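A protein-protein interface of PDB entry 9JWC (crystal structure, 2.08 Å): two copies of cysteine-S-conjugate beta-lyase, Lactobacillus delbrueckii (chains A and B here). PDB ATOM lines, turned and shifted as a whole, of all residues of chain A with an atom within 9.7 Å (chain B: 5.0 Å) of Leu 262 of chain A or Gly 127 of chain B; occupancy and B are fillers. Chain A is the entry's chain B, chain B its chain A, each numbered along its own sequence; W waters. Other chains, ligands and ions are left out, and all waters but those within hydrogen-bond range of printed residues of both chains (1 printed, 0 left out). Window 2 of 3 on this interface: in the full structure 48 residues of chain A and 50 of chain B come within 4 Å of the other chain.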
ATOM      1  N   PRO A  95     -10.860 -18.908   9.696  1.00  0.00           N
ATOM      2  CA  PRO A  95     -11.369 -20.007  10.535  1.00  0.00           C
ATOM      3  C   PRO A  95     -11.865 -21.195   9.727  1.00  0.00           C
ATOM      4  O   PRO A  95     -11.714 -22.337  10.167  1.00  0.00           O
ATOM      5  CB  PRO A  95     -12.510 -19.346  11.323  1.00  0.00           C
ATOM      6  CG  PRO A  95     -12.148 -17.924  11.368  1.00  0.00           C
ATOM      7  CD  PRO A  95     -11.484 -17.620  10.066  1.00  0.00           C
ATOM      8  N   ALA A  99     -10.472 -24.967  10.128  1.00  0.00           N
ATOM      9  CA  ALA A  99     -11.321 -26.134  10.360  1.00  0.00           C
ATOM     10  C   ALA A  99     -11.113 -27.198   9.294  1.00  0.00           C
ATOM     11  O   ALA A  99     -11.139 -28.398   9.592  1.00  0.00           O
ATOM     12  CB  ALA A  99     -12.796 -25.715  10.406  1.00  0.00           C
ATOM     13  N   ARG A 102      -7.990 -29.173   9.855  1.00  0.00           N
ATOM     14  CA  ARG A 102      -8.150 -30.218  10.858  1.00  0.00           C
ATOM     15  C   ARG A 102      -9.006 -31.359  10.322  1.00  0.00           C
ATOM     16  O   ARG A 102      -8.729 -32.530  10.596  1.00  0.00           O
ATOM     17  CB  ARG A 102      -8.756 -29.643  12.142  1.00  0.00           C
ATOM     18  CG  ARG A 102      -7.812 -28.728  12.930  1.00  0.00           C
ATOM     19  CD  ARG A 102      -8.356 -28.402  14.340  1.00  0.00           C
ATOM     20  NE  ARG A 102      -9.639 -27.706  14.240  1.00  0.00           N
ATOM     21  CZ  ARG A 102      -9.776 -26.414  13.976  1.00  0.00           C
ATOM     22  NH1 ARG A 102      -8.703 -25.639  13.833  1.00  0.00           N
ATOM     23  NH2 ARG A 102     -10.995 -25.890  13.874  1.00  0.00           N
ATOM     24  N   GLN A 103     -10.030 -31.041   9.528  1.00  0.00           N
ATOM     25  CA  GLN A 103     -10.965 -32.076   9.099  1.00  0.00           C
ATOM     26  C   GLN A 103     -10.415 -32.904   7.946  1.00  0.00           C
ATOM     27  O   GLN A 103     -10.664 -34.111   7.870  1.00  0.00           O
ATOM     28  CB  GLN A 103     -12.294 -31.443   8.702  1.00  0.00           C
ATOM     29  CG  GLN A 103     -13.381 -32.446   8.272  1.00  0.00           C
ATOM     30  CD  GLN A 103     -14.016 -33.175   9.448  1.00  0.00           C
ATOM     31  OE1 GLN A 103     -13.357 -33.925  10.163  1.00  0.00           O
ATOM     32  NE2 GLN A 103     -15.321 -32.963   9.639  1.00  0.00           N
ATOM     33  N   ALA A 254     -20.718 -31.419   3.409  1.00  0.00           N
ATOM     34  CA  ALA A 254     -21.320 -31.783   4.681  1.00  0.00           C
ATOM     35  C   ALA A 254     -20.261 -31.987   5.752  1.00  0.00           C
ATOM     36  O   ALA A 254     -20.487 -31.657   6.921  1.00  0.00           O
ATOM     37  CB  ALA A 254     -22.166 -33.045   4.514  1.00  0.00           C
ATOM     38  N   ARG A 255     -19.098 -32.515   5.370  1.00  0.00           N
ATOM     39  CA  ARG A 255     -18.036 -32.706   6.352  1.00  0.00           C
ATOM     40  C   ARG A 255     -17.434 -31.376   6.768  1.00  0.00           C
ATOM     41  O   ARG A 255     -17.128 -31.165   7.949  1.00  0.00           O
ATOM     42  CB  ARG A 255     -16.966 -33.630   5.780  1.00  0.00           C
ATOM     43  CG  ARG A 255     -17.445 -35.069   5.629  1.00  0.00           C
ATOM     44  CD  ARG A 255     -16.403 -35.893   4.907  1.00  0.00           C
ATOM     45  NE  ARG A 255     -15.145 -35.929   5.654  1.00  0.00           N
ATOM     46  CZ  ARG A 255     -13.953 -36.090   5.095  1.00  0.00           C
ATOM     47  NH1 ARG A 255     -13.853 -36.242   3.779  1.00  0.00           N
ATOM     48  NH2 ARG A 255     -12.859 -36.118   5.853  1.00  0.00           N
ATOM     49  N   ALA A 256     -17.255 -30.463   5.813  1.00  0.00           N
ATOM     50  CA  ALA A 256     -16.764 -29.141   6.178  1.00  0.00           C
ATOM     51  C   ALA A 256     -17.764 -28.426   7.072  1.00  0.00           C
ATOM     52  O   ALA A 256     -17.383 -27.804   8.074  1.00  0.00           O
ATOM     53  CB  ALA A 256     -16.460 -28.323   4.920  1.00  0.00           C
ATOM     54  N   GLU A 257     -19.056 -28.516   6.742  1.00  0.00           N
ATOM     55  CA  GLU A 257     -20.069 -27.911   7.602  1.00  0.00           C
ATOM     56  C   GLU A 257     -19.996 -28.469   9.019  1.00  0.00           C
ATOM     57  O   GLU A 257     -20.108 -27.721   9.995  1.00  0.00           O
ATOM     58  CB  GLU A 257     -21.458 -28.134   7.014  1.00  0.00           C
ATOM     59  CG  GLU A 257     -22.581 -27.628   7.898  1.00  0.00           C
ATOM     60  CD  GLU A 257     -23.952 -27.855   7.289  1.00  0.00           C
ATOM     61  OE1 GLU A 257     -24.852 -27.026   7.529  1.00  0.00           O
ATOM     62  OE2 GLU A 257     -24.125 -28.861   6.579  1.00  0.00           O
ATOM     63  N   GLU A 258     -19.828 -29.786   9.156  1.00  0.00           N
ATOM     64  CA  GLU A 258     -19.727 -30.379  10.486  1.00  0.00           C
ATOM     65  C   GLU A 258     -18.501 -29.858  11.230  1.00  0.00           C
ATOM     66  O   GLU A 258     -18.565 -29.587  12.436  1.00  0.00           O
ATOM     67  CB  GLU A 258     -19.693 -31.905  10.382  1.00  0.00           C
ATOM     68  CG  GLU A 258     -19.915 -32.600  11.706  1.00  0.00           C
ATOM     69  CD  GLU A 258     -20.452 -34.021  11.559  1.00  0.00           C
ATOM     70  OE1 GLU A 258     -20.658 -34.486  10.416  1.00  0.00           O
ATOM     71  OE2 GLU A 258     -20.691 -34.660  12.611  1.00  0.00           O
ATOM     72  N   SER A 259     -17.373 -29.717  10.524  1.00  0.00           N
ATOM     73  CA  SER A 259     -16.172 -29.164  11.136  1.00  0.00           C
ATOM     74  C   SER A 259     -16.353 -27.701  11.533  1.00  0.00           C
ATOM     75  O   SER A 259     -15.747 -27.251  12.511  1.00  0.00           O
ATOM     76  CB  SER A 259     -14.996 -29.286  10.184  1.00  0.00           C
ATOM     77  OG  SER A 259     -14.991 -28.198   9.281  1.00  0.00           O
ATOM     78  N   PHE A 260     -17.139 -26.935  10.768  1.00  0.00           N
ATOM     79  CA  PHE A 260     -17.424 -25.555  11.160  1.00  0.00           C
ATOM     80  C   PHE A 260     -18.215 -25.529  12.458  1.00  0.00           C
ATOM     81  O   PHE A 260     -17.910 -24.762  13.375  1.00  0.00           O
ATOM     82  CB  PHE A 260     -18.217 -24.826  10.068  1.00  0.00           C
ATOM     83  CG  PHE A 260     -17.512 -24.711   8.734  1.00  0.00           C
ATOM     84  CD1 PHE A 260     -16.147 -24.909   8.608  1.00  0.00           C
ATOM     85  CD2 PHE A 260     -18.246 -24.397   7.592  1.00  0.00           C
ATOM     86  CE1 PHE A 260     -15.524 -24.796   7.368  1.00  0.00           C
ATOM     87  CE2 PHE A 260     -17.632 -24.286   6.361  1.00  0.00           C
ATOM     88  CZ  PHE A 260     -16.261 -24.484   6.247  1.00  0.00           C
ATOM     89  N   PHE A 261     -19.261 -26.354  12.537  1.00  0.00           N
ATOM     90  CA  PHE A 261     -20.084 -26.385  13.736  1.00  0.00           C
ATOM     91  C   PHE A 261     -19.268 -26.797  14.944  1.00  0.00           C
ATOM     92  O   PHE A 261     -19.360 -26.174  16.007  1.00  0.00           O
ATOM     93  CB  PHE A 261     -21.257 -27.336  13.525  1.00  0.00           C
ATOM     94  CG  PHE A 261     -22.413 -26.671  12.874  1.00  0.00           C
ATOM     95  CD1 PHE A 261     -22.905 -25.482  13.393  1.00  0.00           C
ATOM     96  CD2 PHE A 261     -22.977 -27.190  11.723  1.00  0.00           C
ATOM     97  CE1 PHE A 261     -23.956 -24.835  12.791  1.00  0.00           C
ATOM     98  CE2 PHE A 261     -24.035 -26.551  11.114  1.00  0.00           C
ATOM     99  CZ  PHE A 261     -24.522 -25.369  11.646  1.00  0.00           C
ATOM    100  N   LEU A 262     -18.434 -27.826  14.779  1.00  0.00           N
ATOM    101  CA  LEU A 262     -17.608 -28.328  15.872  1.00  0.00           C
ATOM    102  C   LEU A 262     -16.625 -27.271  16.364  1.00  0.00           C
ATOM    103  O   LEU A 262     -16.389 -27.142  17.572  1.00  0.00           O
ATOM    104  CB  LEU A 262     -16.858 -29.570  15.398  1.00  0.00           C
ATOM    105  CG  LEU A 262     -17.158 -30.925  16.019  1.00  0.00           C
ATOM    106  CD1 LEU A 262     -16.003 -31.872  15.732  1.00  0.00           C
ATOM    107  CD2 LEU A 262     -17.408 -30.799  17.512  1.00  0.00           C
ATOM    108  N   ALA A 263     -16.047 -26.499  15.442  1.00  0.00           N
ATOM    109  CA  ALA A 263     -15.069 -25.478  15.806  1.00  0.00           C
ATOM    110  C   ALA A 263     -15.714 -24.253  16.441  1.00  0.00           C
ATOM    111  O   ALA A 263     -15.036 -23.501  17.144  1.00  0.00           O
ATOM    112  CB  ALA A 263     -14.289 -25.044  14.563  1.00  0.00           C
ATOM    113  N   GLY A 264     -16.994 -24.020  16.181  1.00  0.00           N
ATOM    114  CA  GLY A 264     -17.676 -22.837  16.650  1.00  0.00           C
ATOM    115  C   GLY A 264     -17.725 -21.703  15.659  1.00  0.00           C
ATOM    116  O   GLY A 264     -17.820 -20.548  16.076  1.00  0.00           O
ATOM    117  N   ILE A 265     -17.642 -21.990  14.362  1.00  0.00           N
ATOM    118  CA  ILE A 265     -17.677 -20.963  13.333  1.00  0.00           C
ATOM    119  C   ILE A 265     -18.812 -21.197  12.347  1.00  0.00           C
ATOM    120  O   ILE A 265     -18.829 -20.591  11.279  1.00  0.00           O
ATOM    121  CB  ILE A 265     -16.329 -20.868  12.588  1.00  0.00           C
ATOM    122  CG1 ILE A 265     -16.056 -22.179  11.838  1.00  0.00           C
ATOM    123  CG2 ILE A 265     -15.185 -20.551  13.541  1.00  0.00           C
ATOM    124  CD1 ILE A 265     -14.938 -22.095  10.823  1.00  0.00           C
ATOM    125  N   GLY A 266     -19.753 -22.080  12.677  1.00  0.00           N
ATOM    126  CA  GLY A 266     -20.805 -22.439  11.741  1.00  0.00           C
ATOM    127  C   GLY A 266     -22.088 -21.653  11.924  1.00  0.00           C
ATOM    128  O   GLY A 266     -23.006 -21.746  11.103  1.00  0.00           O
ATOM    129  N   GLU A 267     -22.156 -20.935  13.045  1.00  0.00           N
ATOM    130  CA  GLU A 267     -23.389 -20.210  13.432  1.00  0.00           C
ATOM    131  C   GLU A 267     -23.268 -18.684  13.211  1.00  0.00           C
ATOM    132  O   GLU A 267     -22.347 -18.101  13.718  1.00  0.00           O
ATOM    133  CB  GLU A 267     -23.738 -20.541  14.882  1.00  0.00           C
ATOM    134  CG  GLU A 267     -24.892 -19.769  15.483  1.00  0.00           C
ATOM    135  CD  GLU A 267     -25.031 -19.916  16.993  1.00  0.00           C
ATOM    136  OE1 GLU A 267     -25.125 -21.063  17.462  1.00  0.00           O
ATOM    137  OE2 GLU A 267     -25.036 -18.883  17.697  1.00  0.00           O
ATOM    138  N   SER B  98     -14.740 -26.865  23.130  1.00  0.00           N
ATOM    139  CA  SER B  98     -14.338 -27.712  22.011  1.00  0.00           C
ATOM    140  C   SER B  98     -12.861 -27.502  21.687  1.00  0.00           C
ATOM    141  O   SER B  98     -12.116 -28.470  21.493  1.00  0.00           O
ATOM    142  CB  SER B  98     -15.242 -27.425  20.802  1.00  0.00           C
ATOM    143  OG  SER B  98     -14.905 -28.227  19.686  1.00  0.00           O
ATOM    144  N   ARG B 102      -9.626 -30.233  22.290  1.00  0.00           N
ATOM    145  CA  ARG B 102      -8.591 -30.564  21.313  1.00  0.00           C
ATOM    146  C   ARG B 102      -7.195 -30.227  21.828  1.00  0.00           C
ATOM    147  O   ARG B 102      -6.232 -30.947  21.538  1.00  0.00           O
ATOM    148  CB  ARG B 102      -8.838 -29.824  19.995  1.00  0.00           C
ATOM    149  CG  ARG B 102     -10.055 -30.308  19.207  1.00  0.00           C
ATOM    150  CD  ARG B 102     -10.067 -29.712  17.806  1.00  0.00           C
ATOM    151  NE  ARG B 102     -10.171 -28.255  17.820  1.00  0.00           N
ATOM    152  CZ  ARG B 102     -11.304 -27.584  17.987  1.00  0.00           C
ATOM    153  NH1 ARG B 102     -12.456 -28.234  18.155  1.00  0.00           N
ATOM    154  NH2 ARG B 102     -11.286 -26.253  17.999  1.00  0.00           N
ATOM    155  N   TYR B 122     -21.769 -33.382  25.354  1.00  0.00           N
ATOM    156  CA  TYR B 122     -21.531 -34.630  24.638  1.00  0.00           C
ATOM    157  C   TYR B 122     -21.116 -34.366  23.199  1.00  0.00           C
ATOM    158  O   TYR B 122     -20.249 -35.061  22.658  1.00  0.00           O
ATOM    159  CB  TYR B 122     -22.778 -35.505  24.661  1.00  0.00           C
ATOM    160  CG  TYR B 122     -23.436 -35.591  26.006  1.00  0.00           C
ATOM    161  CD1 TYR B 122     -22.724 -36.040  27.115  1.00  0.00           C
ATOM    162  CD2 TYR B 122     -24.767 -35.242  26.171  1.00  0.00           C
ATOM    163  CE1 TYR B 122     -23.314 -36.129  28.340  1.00  0.00           C
ATOM    164  CE2 TYR B 122     -25.378 -35.329  27.417  1.00  0.00           C
ATOM    165  CZ  TYR B 122     -24.646 -35.776  28.493  1.00  0.00           C
ATOM    166  OH  TYR B 122     -25.238 -35.872  29.723  1.00  0.00           O
ATOM    167  N   SER B 123     -21.737 -33.375  22.558  1.00  0.00           N
ATOM    168  CA  SER B 123     -21.411 -33.078  21.169  1.00  0.00           C
ATOM    169  C   SER B 123     -19.950 -32.689  21.023  1.00  0.00           C
ATOM    170  O   SER B 123     -19.261 -33.164  20.115  1.00  0.00           O
ATOM    171  CB  SER B 123     -22.321 -31.967  20.639  1.00  0.00           C
ATOM    172  OG  SER B 123     -23.671 -32.393  20.638  1.00  0.00           O
ATOM    173  N   VAL B 124     -19.460 -31.818  21.902  1.00  0.00           N
ATOM    174  CA  VAL B 124     -18.086 -31.368  21.738  1.00  0.00           C
ATOM    175  C   VAL B 124     -17.089 -32.410  22.224  1.00  0.00           C
ATOM    176  O   VAL B 124     -15.951 -32.447  21.738  1.00  0.00           O
ATOM    177  CB  VAL B 124     -17.858 -30.016  22.437  1.00  0.00           C
ATOM    178  CG1 VAL B 124     -18.794 -28.960  21.856  1.00  0.00           C
ATOM    179  CG2 VAL B 124     -18.018 -30.135  23.945  1.00  0.00           C
ATOM    180  N   ILE B 125     -17.457 -33.253  23.191  1.00  0.00           N
ATOM    181  CA  ILE B 125     -16.530 -34.308  23.607  1.00  0.00           C
ATOM    182  C   ILE B 125     -16.458 -35.391  22.537  1.00  0.00           C
ATOM    183  O   ILE B 125     -15.382 -35.707  22.010  1.00  0.00           O
ATOM    184  CB  ILE B 125     -16.941 -34.891  24.968  1.00  0.00           C
ATOM    185  CG1 ILE B 125     -16.715 -33.857  26.073  1.00  0.00           C
ATOM    186  CG2 ILE B 125     -16.133 -36.150  25.272  1.00  0.00           C
ATOM    187  CD1 ILE B 125     -17.371 -34.221  27.388  1.00  0.00           C
ATOM    188  N   GLU B 126     -17.616 -35.953  22.188  1.00  0.00           N
ATOM    189  CA  GLU B 126     -17.672 -37.070  21.251  1.00  0.00           C
ATOM    190  C   GLU B 126     -17.388 -36.615  19.824  1.00  0.00           C
ATOM    191  O   GLU B 126     -16.760 -37.345  19.044  1.00  0.00           O
ATOM    192  CB  GLU B 126     -19.042 -37.744  21.342  1.00  0.00           C
ATOM    193  CG  GLU B 126     -19.353 -38.221  22.760  1.00  0.00           C
ATOM    194  CD  GLU B 126     -20.710 -38.890  22.907  1.00  0.00           C
ATOM    195  OE1 GLU B 126     -20.833 -39.744  23.807  1.00  0.00           O
ATOM    196  OE2 GLU B 126     -21.648 -38.561  22.153  1.00  0.00           O
ATOM    197  N   GLY B 127     -17.845 -35.415  19.465  1.00  0.00           N
ATOM    198  CA  GLY B 127     -17.580 -34.904  18.133  1.00  0.00           C
ATOM    199  C   GLY B 127     -16.098 -34.719  17.875  1.00  0.00           C
ATOM    200  O   GLY B 127     -15.641 -34.840  16.736  1.00  0.00           O
ATOM    201  N   ASN B 128     -15.325 -34.431  18.922  1.00  0.00           N
ATOM    202  CA  ASN B 128     -13.882 -34.334  18.781  1.00  0.00           C
ATOM    203  C   ASN B 128     -13.178 -35.665  18.987  1.00  0.00           C
ATOM    204  O   ASN B 128     -11.950 -35.693  19.018  1.00  0.00           O
ATOM    205  CB  ASN B 128     -13.310 -33.288  19.749  1.00  0.00           C
ATOM    206  CG  ASN B 128     -13.538 -31.865  19.267  1.00  0.00           C
ATOM    207  OD1 ASN B 128     -12.997 -31.458  18.238  1.00  0.00           O
ATOM    208  ND2 ASN B 128     -14.357 -31.108  19.999  1.00  0.00           N
ATOM    209  N   GLY B 129     -13.911 -36.765  19.132  1.00  0.00           N
ATOM    210  CA  GLY B 129     -13.252 -38.046  19.295  1.00  0.00           C
ATOM    211  C   GLY B 129     -12.672 -38.282  20.664  1.00  0.00           C
ATOM    212  O   GLY B 129     -11.669 -38.990  20.801  1.00  0.00           O
HETATM  213  O   HOH W   1     -13.396 -24.774  18.891  1.00  0.00           O
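The backbone carbonyl oxygen (O) of Leu 262 of chain A sits at hydrogen-bond distance from the side-chain hydroxyl (OG) of Ser 98 of chain B, at 2.8 Å.
Leu 262 of chain A touches four residues of chain B.
Of the printed residues of chain A, Ser 98 of chain B touches Leu 262 (2.8 Å).
Printed residues of chain A within 4 Å of Arg 102 of chain B: Arg 102.
Of the printed residues of chain A, Ser 123 of chain B touches Leu 262 (3.98 Å).
Gly 127 of chain B touches just one residue of chain A: Leu 262 (3.2 Å).
The nearest residue of chain B that does not touch Leu 262 of chain A is Arg 102 of chain B (4.1 Å).
The nearest residue of chain A that does not touch Gly 127 of chain B is Glu 258 of chain A (6.3 Å).
The nearest printed residue of chain A that does not touch Arg 102 of chain B is Leu 262 of chain A (4.1 Å).
Hydrophobic or aromatic side chains of chain A within 4 Å of the printed part of chain B: Leu 262.
Of the 10 printed residues of chain B, 5 touch a printed residue of chain A.
Among the printed residues, no Asp or Glu carboxylate lies within 4 Å of a Lys or Arg side-chain nitrogen of the other chain.
Water W1 lies within hydrogen-bond range of O of Ala 263 of chain A and NH2 of Arg 102 of chain B.
The guanidinium group of Arg 102 of chain B sits at hydrogen-bond distance from the side-chain hydroxyl of Ser 98 of chain B, 2.9 Å away.
The side-chain amide nitrogen (ND2) of Asn 128 of chain B is in hydrogen-bond range of the side-chain hydroxyl (OG) of Ser 98 of chain B, 2.9 Å away.
The guanidinium group (NH1) of Arg 102 of chain B is in hydrogen-bond range of the side-chain amide oxygen (OD1) of Asn 128 of chain B, 3.3 Å away.
The backbone carbonyl oxygen (O) of Val 124 of chain B sits at hydrogen-bond distance from the side-chain amide nitrogen (ND2) of Asn 128 of chain B (2.7 Å).
Arg 102 of chain B touches its own counterpart, Arg 102 of chain A.
Among the printed residues, merely in contact across the chains: Arg 102 of chain A with Arg 102 of chain B (3.7 Å), Leu 262 of chain A with Ser 123 of chain B (3.98 Å), Leu 262 of chain A with Gly 127 of chain B (3.2 Å) and Leu 262 of chain A with Asn 128 of chain B (3.9 Å).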
